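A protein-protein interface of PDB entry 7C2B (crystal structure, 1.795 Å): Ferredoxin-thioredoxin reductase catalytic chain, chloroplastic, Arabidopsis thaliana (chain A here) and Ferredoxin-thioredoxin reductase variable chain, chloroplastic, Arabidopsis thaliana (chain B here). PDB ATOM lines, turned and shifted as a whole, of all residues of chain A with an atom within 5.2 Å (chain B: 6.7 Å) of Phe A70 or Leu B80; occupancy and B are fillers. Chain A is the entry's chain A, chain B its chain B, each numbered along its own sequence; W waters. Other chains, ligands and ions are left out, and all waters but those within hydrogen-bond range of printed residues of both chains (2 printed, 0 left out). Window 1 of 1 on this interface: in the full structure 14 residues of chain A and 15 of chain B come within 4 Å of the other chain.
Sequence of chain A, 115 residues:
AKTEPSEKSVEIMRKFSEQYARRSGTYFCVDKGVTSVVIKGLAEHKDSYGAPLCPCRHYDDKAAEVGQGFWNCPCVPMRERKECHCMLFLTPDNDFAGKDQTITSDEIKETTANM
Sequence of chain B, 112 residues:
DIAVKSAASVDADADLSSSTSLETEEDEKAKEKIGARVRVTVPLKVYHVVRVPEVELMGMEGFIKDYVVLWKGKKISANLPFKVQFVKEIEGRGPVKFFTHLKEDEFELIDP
OE1 of Gln A68 is in hydrogen-bond range of N of Phe A70, 3.0 Å away.
The backbone carbonyl oxygen of Phe A70 lies within hydrogen-bond range of the backbone NH of Val A76 (3.0 Å).
The backbone carbonyl oxygen of Phe B82 is in hydrogen-bond range of the backbone NH of Leu B102 (2.8 Å).
The side-chain amino group (NZ) of Lys B103 lies within salt-bridge range of the side-chain carboxylate (OE2) of Glu B106, at 3.6 Å.
Printed residues of chain A that touch a printed residue of chain B: Glu A65, Gln A68, Phe A70, Trp A71, Val A76 and Arg A81.
Printed residues of chain B that touch a printed residue of chain A: Ile B76, Ser B77, Ala B78, Asn B79, Leu B80, His B101, Leu B102 and Glu B106.
Hydrophobic or aromatic side chains of chain B within 4 Å of the printed part of chain A: Ile B76, Ala B78, Leu B80, His B101 and Leu B102.
Among the printed residues, 14 pairs touch across the chains.
Among the printed residues, Asp or Glu carboxylates within 4 Å of a Lys or Arg side-chain nitrogen of the other chain: Arg A81 with Glu B106.
Ile B76 touches Glu A65 (CA to OE2, 3.5 Å).
Gln A68 touches Ile B76.
CG of Phe A70 touches CB of Ala B78, at 3.5 Å.
Phe A70 touches Asn B79 (CZ to OD1, 3.3 Å).
Phe A70 touches Leu B80.
Trp A71 touches Ala B78.
Asn B79 touches Trp A71.
His B101 touches Val A76.
CD2 of Leu B80 touches NH2 of Arg A81, at 3.6 Å.
Leu B102 touches Arg A81 (CD2 to NH2, 3.8 Å).
Water W2 lies within hydrogen-bond range of O of His B101 (2.7 Å) and NE of Arg A81 (2.8 Å).
Water W1 lies within hydrogen-bond range of the side-chain carboxylate (OE1) of Glu A65 (2.8 Å), the side-chain amide oxygen (OE1) of Gln A68 (2.9 Å), the backbone NH (N) of Ala B78 (3.1 Å) and the backbone NH (N) of Ser B77 (3.5 Å).
Of chain A, only Phe A70 and Arg A81 come within 4 Å of Leu B80.
Of the printed residues of chain B, Glu A65 touches Ile B76 and Ser B77.
Printed residues of chain B within 4 Å of Trp A71: Ser B77, Ala B78 and Asn B79.
Of the printed residues of chain A, Leu B102 touches Arg A81.
Of the printed residues of chain A, His B101 touches Val A76 and Arg A81.
Arg A79 touches none of the printed residues of chain B.
Pro B81 touches none of the printed residues of chain A.
The nearest residue of chain A that does not touch Leu B80 is Pro A77 (4.3 Å).
The nearest printed residue of chain A that does not touch Leu B102 is Phe A70 (7.0 Å).
OG of Ser B77 is in hydrogen-bond range of OE2 of Glu A65 (2.7 Å).
NE1 of Trp A71 sits at hydrogen-bond distance from O of Ser B77.
The backbone carbonyl oxygen (O) of His B101 sits at hydrogen-bond distance from the guanidinium group (NH2) of Arg A81 (3.0 Å).
The side-chain carboxylate (OE1) of Glu B106 is in salt-bridge range of the guanidinium group (NH2) of Arg A81, 2.8 Å away.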
ATOM      1  N   GLU A  65      28.264  -3.042  17.545  1.00  0.00           N
ATOM      2  CA  GLU A  65      26.809  -2.961  17.630  1.00  0.00           C
ATOM      3  C   GLU A  65      26.203  -2.441  16.325  1.00  0.00           C
ATOM      4  O   GLU A  65      25.175  -2.949  15.869  1.00  0.00           O
ATOM      5  CB  GLU A  65      26.412  -2.075  18.809  1.00  0.00           C
ATOM      6  CG  GLU A  65      26.800  -2.665  20.168  1.00  0.00           C
ATOM      7  CD  GLU A  65      25.819  -3.716  20.658  1.00  0.00           C
ATOM      8  OE1 GLU A  65      24.796  -3.958  19.980  1.00  0.00           O
ATOM      9  OE2 GLU A  65      26.064  -4.299  21.738  1.00  0.00           O
ATOM     10  N   GLN A  68      26.408  -5.422  13.830  1.00  0.00           N
ATOM     11  CA  GLN A  68      25.506  -6.536  14.078  1.00  0.00           C
ATOM     12  C   GLN A  68      24.040  -6.113  13.949  1.00  0.00           C
ATOM     13  O   GLN A  68      23.223  -6.861  13.403  1.00  0.00           O
ATOM     14  CB  GLN A  68      25.803  -7.144  15.446  1.00  0.00           C
ATOM     15  CG  GLN A  68      25.207  -8.507  15.629  1.00  0.00           C
ATOM     16  CD  GLN A  68      23.782  -8.393  16.080  1.00  0.00           C
ATOM     17  OE1 GLN A  68      23.426  -7.427  16.761  1.00  0.00           O
ATOM     18  NE2 GLN A  68      22.945  -9.347  15.682  1.00  0.00           N
ATOM     19  N   GLY A  69      23.689  -4.928  14.443  1.00  0.00           N
ATOM     20  CA  GLY A  69      22.436  -4.290  14.068  1.00  0.00           C
ATOM     21  C   GLY A  69      21.228  -4.567  14.946  1.00  0.00           C
ATOM     22  O   GLY A  69      20.168  -3.980  14.695  1.00  0.00           O
ATOM     23  N   PHE A  70      21.351  -5.430  15.963  1.00  0.00           N
ATOM     24  CA  PHE A  70      20.197  -5.784  16.794  1.00  0.00           C
ATOM     25  C   PHE A  70      19.544  -4.544  17.393  1.00  0.00           C
ATOM     26  O   PHE A  70      18.312  -4.429  17.412  1.00  0.00           O
ATOM     27  CB  PHE A  70      20.638  -6.754  17.899  1.00  0.00           C
ATOM     28  CG  PHE A  70      19.506  -7.308  18.758  1.00  0.00           C
ATOM     29  CD1 PHE A  70      18.998  -6.574  19.827  1.00  0.00           C
ATOM     30  CD2 PHE A  70      18.994  -8.569  18.520  1.00  0.00           C
ATOM     31  CE1 PHE A  70      17.977  -7.083  20.642  1.00  0.00           C
ATOM     32  CE2 PHE A  70      17.988  -9.101  19.332  1.00  0.00           C
ATOM     33  CZ  PHE A  70      17.474  -8.350  20.399  1.00  0.00           C
ATOM     34  N   TRP A  71      20.350  -3.605  17.873  1.00  0.00           N
ATOM     35  CA  TRP A  71      19.835  -2.431  18.555  1.00  0.00           C
ATOM     36  C   TRP A  71      19.774  -1.209  17.648  1.00  0.00           C
ATOM     37  O   TRP A  71      19.542  -0.107  18.145  1.00  0.00           O
ATOM     38  CB  TRP A  71      20.667  -2.120  19.797  1.00  0.00           C
ATOM     39  CG  TRP A  71      20.408  -3.070  20.912  1.00  0.00           C
ATOM     40  CD1 TRP A  71      21.306  -3.942  21.468  1.00  0.00           C
ATOM     41  CD2 TRP A  71      19.167  -3.270  21.609  1.00  0.00           C
ATOM     42  NE1 TRP A  71      20.704  -4.659  22.464  1.00  0.00           N
ATOM     43  CE2 TRP A  71      19.388  -4.281  22.563  1.00  0.00           C
ATOM     44  CE3 TRP A  71      17.893  -2.697  21.509  1.00  0.00           C
ATOM     45  CZ2 TRP A  71      18.386  -4.727  23.430  1.00  0.00           C
ATOM     46  CZ3 TRP A  71      16.886  -3.142  22.361  1.00  0.00           C
ATOM     47  CH2 TRP A  71      17.138  -4.145  23.314  1.00  0.00           C
ATOM     48  N   ASN A  72      20.003  -1.369  16.344  1.00  0.00           N
ATOM     49  CA  ASN A  72      19.780  -0.264  15.417  1.00  0.00           C
ATOM     50  C   ASN A  72      18.286  -0.026  15.236  1.00  0.00           C
ATOM     51  O   ASN A  72      17.539  -0.940  14.882  1.00  0.00           O
ATOM     52  CB  ASN A  72      20.416  -0.542  14.058  1.00  0.00           C
ATOM     53  CG  ASN A  72      20.484   0.707  13.193  1.00  0.00           C
ATOM     54  OD1 ASN A  72      20.893   1.761  13.670  1.00  0.00           O
ATOM     55  ND2 ASN A  72      20.047   0.611  11.940  1.00  0.00           N
ATOM     56  N   PRO A  74      14.775   0.728  13.733  1.00  0.00           N
ATOM     57  CA  PRO A  74      13.936   0.004  14.691  1.00  0.00           C
ATOM     58  C   PRO A  74      14.598  -1.284  15.118  1.00  0.00           C
ATOM     59  O   PRO A  74      14.971  -2.095  14.264  1.00  0.00           O
ATOM     60  CB  PRO A  74      12.655  -0.285  13.910  1.00  0.00           C
ATOM     61  CG  PRO A  74      13.089  -0.320  12.449  1.00  0.00           C
ATOM     62  CD  PRO A  74      14.287   0.604  12.342  1.00  0.00           C
ATOM     63  N   CYS A  75      14.754  -1.460  16.427  1.00  0.00           N
ATOM     64  CA  CYS A  75      15.509  -2.596  16.944  1.00  0.00           C
ATOM     65  C   CYS A  75      14.724  -3.902  16.772  1.00  0.00           C
ATOM     66  O   CYS A  75      13.531  -3.916  16.462  1.00  0.00           O
ATOM     67  CB  CYS A  75      15.855  -2.375  18.416  1.00  0.00           C
ATOM     68  SG  CYS A  75      14.348  -2.196  19.454  1.00  0.00           S
ATOM     69  N   VAL A  76      15.400  -5.023  17.020  1.00  0.00           N
ATOM     70  CA  VAL A  76      14.738  -6.321  16.898  1.00  0.00           C
ATOM     71  C   VAL A  76      13.513  -6.439  17.805  1.00  0.00           C
ATOM     72  O   VAL A  76      12.473  -6.935  17.333  1.00  0.00           O
ATOM     73  CB  VAL A  76      15.752  -7.455  17.111  1.00  0.00           C
ATOM     74  CG1 VAL A  76      15.025  -8.747  17.385  1.00  0.00           C
ATOM     75  CG2 VAL A  76      16.616  -7.592  15.857  1.00  0.00           C
ATOM     76  N   PRO A  77      13.553  -6.032  19.080  1.00  0.00           N
ATOM     77  CA  PRO A  77      12.324  -6.144  19.890  1.00  0.00           C
ATOM     78  C   PRO A  77      11.160  -5.358  19.325  1.00  0.00           C
ATOM     79  O   PRO A  77      10.015  -5.806  19.443  1.00  0.00           O
ATOM     80  CB  PRO A  77      12.753  -5.614  21.268  1.00  0.00           C
ATOM     81  CG  PRO A  77      14.203  -6.013  21.354  1.00  0.00           C
ATOM     82  CD  PRO A  77      14.726  -5.754  19.932  1.00  0.00           C
ATOM     83  N   ARG A  79      10.771  -4.565  15.942  1.00  0.00           N
ATOM     84  CA  ARG A  79      10.364  -5.183  14.681  1.00  0.00           C
ATOM     85  C   ARG A  79       9.534  -6.436  14.914  1.00  0.00           C
ATOM     86  O   ARG A  79       8.544  -6.676  14.213  1.00  0.00           O
ATOM     87  CB  ARG A  79      11.594  -5.520  13.840  1.00  0.00           C
ATOM     88  CG  ARG A  79      11.993  -4.421  12.912  1.00  0.00           C
ATOM     89  CD  ARG A  79      13.443  -4.153  13.002  1.00  0.00           C
ATOM     90  NE  ARG A  79      14.258  -5.222  12.454  1.00  0.00           N
ATOM     91  CZ  ARG A  79      15.537  -5.412  12.759  1.00  0.00           C
ATOM     92  NH1 ARG A  79      16.164  -4.615  13.617  1.00  0.00           N
ATOM     93  NH2 ARG A  79      16.196  -6.404  12.190  1.00  0.00           N
ATOM     94  N   ARG A  81       8.321  -7.776  18.200  1.00  0.00           N
ATOM     95  CA  ARG A  81       7.370  -7.802  19.307  1.00  0.00           C
ATOM     96  C   ARG A  81       6.678  -6.468  19.527  1.00  0.00           C
ATOM     97  O   ARG A  81       5.880  -6.356  20.465  1.00  0.00           O
ATOM     98  CB  ARG A  81       8.082  -8.221  20.602  1.00  0.00           C
ATOM     99  CG  ARG A  81       8.884  -9.490  20.435  1.00  0.00           C
ATOM    100  CD  ARG A  81       9.478  -9.969  21.776  1.00  0.00           C
ATOM    101  NE  ARG A  81      10.290 -11.170  21.576  1.00  0.00           N
ATOM    102  CZ  ARG A  81      10.645 -11.997  22.552  1.00  0.00           C
ATOM    103  NH1 ARG A  81      10.265 -11.749  23.804  1.00  0.00           N
ATOM    104  NH2 ARG A  81      11.374 -13.076  22.277  1.00  0.00           N
ATOM    105  N   VAL B  68      23.900 -15.482  18.165  1.00  0.00           N
ATOM    106  CA  VAL B  68      24.828 -14.416  17.825  1.00  0.00           C
ATOM    107  C   VAL B  68      24.995 -13.522  19.042  1.00  0.00           C
ATOM    108  O   VAL B  68      24.075 -12.786  19.418  1.00  0.00           O
ATOM    109  CB  VAL B  68      24.374 -13.623  16.594  1.00  0.00           C
ATOM    110  CG1 VAL B  68      25.392 -12.546  16.268  1.00  0.00           C
ATOM    111  CG2 VAL B  68      24.219 -14.561  15.398  1.00  0.00           C
ATOM    112  N   ILE B  76      28.636  -8.470  21.628  1.00  0.00           N
ATOM    113  CA  ILE B  76      27.591  -7.464  21.478  1.00  0.00           C
ATOM    114  C   ILE B  76      26.428  -7.800  22.417  1.00  0.00           C
ATOM    115  O   ILE B  76      26.399  -8.849  23.057  1.00  0.00           O
ATOM    116  CB  ILE B  76      27.133  -7.313  20.014  1.00  0.00           C
ATOM    117  CG1 ILE B  76      26.946  -8.678  19.350  1.00  0.00           C
ATOM    118  CG2 ILE B  76      28.182  -6.519  19.245  1.00  0.00           C
ATOM    119  CD1 ILE B  76      25.567  -9.277  19.540  1.00  0.00           C
ATOM    120  N   SER B  77      25.473  -6.869  22.522  1.00  0.00           N
ATOM    121  CA  SER B  77      24.552  -6.859  23.656  1.00  0.00           C
ATOM    122  C   SER B  77      23.122  -7.269  23.295  1.00  0.00           C
ATOM    123  O   SER B  77      22.197  -7.009  24.072  1.00  0.00           O
ATOM    124  CB  SER B  77      24.557  -5.474  24.309  1.00  0.00           C
ATOM    125  OG  SER B  77      23.995  -4.495  23.434  1.00  0.00           O
ATOM    126  N   ALA B  78      22.918  -7.892  22.132  1.00  0.00           N
ATOM    127  CA  ALA B  78      21.616  -8.439  21.771  1.00  0.00           C
ATOM    128  C   ALA B  78      21.043  -9.271  22.906  1.00  0.00           C
ATOM    129  O   ALA B  78      21.708 -10.177  23.417  1.00  0.00           O
ATOM    130  CB  ALA B  78      21.752  -9.297  20.509  1.00  0.00           C
ATOM    131  N   ASN B  79      19.805  -8.965  23.314  1.00  0.00           N
ATOM    132  CA  ASN B  79      19.215  -9.657  24.455  1.00  0.00           C
ATOM    133  C   ASN B  79      18.222 -10.751  24.067  1.00  0.00           C
ATOM    134  O   ASN B  79      17.648 -11.392  24.955  1.00  0.00           O
ATOM    135  CB  ASN B  79      18.560  -8.655  25.427  1.00  0.00           C
ATOM    136  CG  ASN B  79      17.354  -7.936  24.840  1.00  0.00           C
ATOM    137  OD1 ASN B  79      16.965  -8.138  23.685  1.00  0.00           O
ATOM    138  ND2 ASN B  79      16.747  -7.076  25.656  1.00  0.00           N
ATOM    139  N   LEU B  80      18.014 -10.993  22.776  1.00  0.00           N
ATOM    140  CA  LEU B  80      17.287 -12.160  22.279  1.00  0.00           C
ATOM    141  C   LEU B  80      18.231 -12.908  21.335  1.00  0.00           C
ATOM    142  O   LEU B  80      18.083 -12.849  20.108  1.00  0.00           O
ATOM    143  CB  LEU B  80      15.989 -11.756  21.574  1.00  0.00           C
ATOM    144  CG  LEU B  80      14.997 -10.929  22.410  1.00  0.00           C
ATOM    145  CD1 LEU B  80      13.870 -10.340  21.546  1.00  0.00           C
ATOM    146  CD2 LEU B  80      14.417 -11.746  23.581  1.00  0.00           C
ATOM    147  N   PRO B  81      19.238 -13.606  21.875  1.00  0.00           N
ATOM    148  CA  PRO B  81      20.354 -14.048  21.019  1.00  0.00           C
ATOM    149  C   PRO B  81      20.092 -15.267  20.151  1.00  0.00           C
ATOM    150  O   PRO B  81      20.869 -15.489  19.212  1.00  0.00           O
ATOM    151  CB  PRO B  81      21.477 -14.348  22.029  1.00  0.00           C
ATOM    152  CG  PRO B  81      20.786 -14.673  23.258  1.00  0.00           C
ATOM    153  CD  PRO B  81      19.529 -13.824  23.302  1.00  0.00           C
ATOM    154  N   PHE B  82      19.051 -16.056  20.413  1.00  0.00           N
ATOM    155  CA  PHE B  82      18.755 -17.246  19.620  1.00  0.00           C
ATOM    156  C   PHE B  82      17.850 -16.885  18.449  1.00  0.00           C
ATOM    157  O   PHE B  82      16.689 -16.517  18.646  1.00  0.00           O
ATOM    158  CB  PHE B  82      18.079 -18.316  20.475  1.00  0.00           C
ATOM    159  CG  PHE B  82      18.973 -18.914  21.533  1.00  0.00           C
ATOM    160  CD1 PHE B  82      19.767 -20.018  21.246  1.00  0.00           C
ATOM    161  CD2 PHE B  82      18.995 -18.397  22.823  1.00  0.00           C
ATOM    162  CE1 PHE B  82      20.586 -20.582  22.219  1.00  0.00           C
ATOM    163  CE2 PHE B  82      19.811 -18.965  23.812  1.00  0.00           C
ATOM    164  CZ  PHE B  82      20.609 -20.057  23.506  1.00  0.00           C
ATOM    165  N   LYS B  83      18.363 -17.021  17.233  1.00  0.00           N
ATOM    166  CA  LYS B  83      17.537 -16.831  16.048  1.00  0.00           C
ATOM    167  C   LYS B  83      16.942 -18.187  15.693  1.00  0.00           C
ATOM    168  O   LYS B  83      17.681 -19.132  15.409  1.00  0.00           O
ATOM    169  CB  LYS B  83      18.357 -16.254  14.896  1.00  0.00           C
ATOM    170  CG  LYS B  83      17.525 -15.795  13.691  1.00  0.00           C
ATOM    171  CD  LYS B  83      18.442 -15.328  12.566  1.00  0.00           C
ATOM    172  CE  LYS B  83      17.765 -15.378  11.211  1.00  0.00           C
ATOM    173  NZ  LYS B  83      18.643 -14.741  10.176  1.00  0.00           N
ATOM    174  N   THR B 100      12.366 -15.798  14.368  1.00  0.00           N
ATOM    175  CA  THR B 100      12.043 -15.012  15.547  1.00  0.00           C
ATOM    176  C   THR B 100      13.226 -15.117  16.497  1.00  0.00           C
ATOM    177  O   THR B 100      13.808 -16.194  16.648  1.00  0.00           O
ATOM    178  CB  THR B 100      10.752 -15.503  16.236  1.00  0.00           C
ATOM    179  OG1 THR B 100       9.612 -15.218  15.409  1.00  0.00           O
ATOM    180  CG2 THR B 100      10.563 -14.818  17.580  1.00  0.00           C
ATOM    181  N   HIS B 101      13.594 -14.000  17.114  1.00  0.00           N
ATOM    182  CA  HIS B 101      14.661 -13.980  18.109  1.00  0.00           C
ATOM    183  C   HIS B 101      14.105 -14.306  19.491  1.00  0.00           C
ATOM    184  O   HIS B 101      13.108 -13.712  19.920  1.00  0.00           O
ATOM    185  CB  HIS B 101      15.336 -12.609  18.118  1.00  0.00           C
ATOM    186  CG  HIS B 101      16.195 -12.353  16.920  1.00  0.00           C
ATOM    187  ND1 HIS B 101      15.692 -11.911  15.710  1.00  0.00           N
ATOM    188  CD2 HIS B 101      17.535 -12.456  16.755  1.00  0.00           C
ATOM    189  CE1 HIS B 101      16.687 -11.758  14.855  1.00  0.00           C
ATOM    190  NE2 HIS B 101      17.814 -12.086  15.464  1.00  0.00           N
ATOM    191  N   LEU B 102      14.756 -15.246  20.187  1.00  0.00           N
ATOM    192  CA  LEU B 102      14.330 -15.682  21.513  1.00  0.00           C
ATOM    193  C   LEU B 102      15.497 -15.614  22.493  1.00  0.00           C
ATOM    194  O   LEU B 102      16.670 -15.620  22.107  1.00  0.00           O
ATOM    195  CB  LEU B 102      13.793 -17.128  21.509  1.00  0.00           C
ATOM    196  CG  LEU B 102      12.681 -17.507  20.538  1.00  0.00           C
ATOM    197  CD1 LEU B 102      12.258 -18.957  20.806  1.00  0.00           C
ATOM    198  CD2 LEU B 102      11.524 -16.568  20.745  1.00  0.00           C
ATOM    199  N   LYS B 103      15.159 -15.547  23.775  1.00  0.00           N
ATOM    200  CA  LYS B 103      16.139 -15.782  24.826  1.00  0.00           C
ATOM    201  C   LYS B 103      15.845 -17.117  25.495  1.00  0.00           C
ATOM    202  O   LYS B 103      14.788 -17.725  25.289  1.00  0.00           O
ATOM    203  CB  LYS B 103      16.159 -14.637  25.850  1.00  0.00           C
ATOM    204  CG  LYS B 103      14.817 -14.263  26.450  1.00  0.00           C
ATOM    205  CD  LYS B 103      15.001 -13.044  27.347  1.00  0.00           C
ATOM    206  CE  LYS B 103      13.679 -12.439  27.754  1.00  0.00           C
ATOM    207  NZ  LYS B 103      12.908 -13.391  28.577  1.00  0.00           N
ATOM    208  N   GLU B 106      12.598 -18.649  27.068  1.00  0.00           N
ATOM    209  CA  GLU B 106      11.359 -18.674  26.306  1.00  0.00           C
ATOM    210  C   GLU B 106      11.134 -19.988  25.570  1.00  0.00           C
ATOM    211  O   GLU B 106      10.094 -20.152  24.925  1.00  0.00           O
ATOM    212  CB  GLU B 106      11.341 -17.495  25.312  1.00  0.00           C
ATOM    213  CG  GLU B 106      11.384 -16.159  26.047  1.00  0.00           C
ATOM    214  CD  GLU B 106      11.501 -14.954  25.127  1.00  0.00           C
ATOM    215  OE1 GLU B 106      12.105 -15.077  24.036  1.00  0.00           O
ATOM    216  OE2 GLU B 106      10.997 -13.878  25.516  1.00  0.00           O
HETATM  217  O   HOH W   1      23.776  -6.514  19.522  1.00  0.00           O
HETATM  218  O   HOH W   2      11.355 -11.803  19.033  1.00  0.00           O
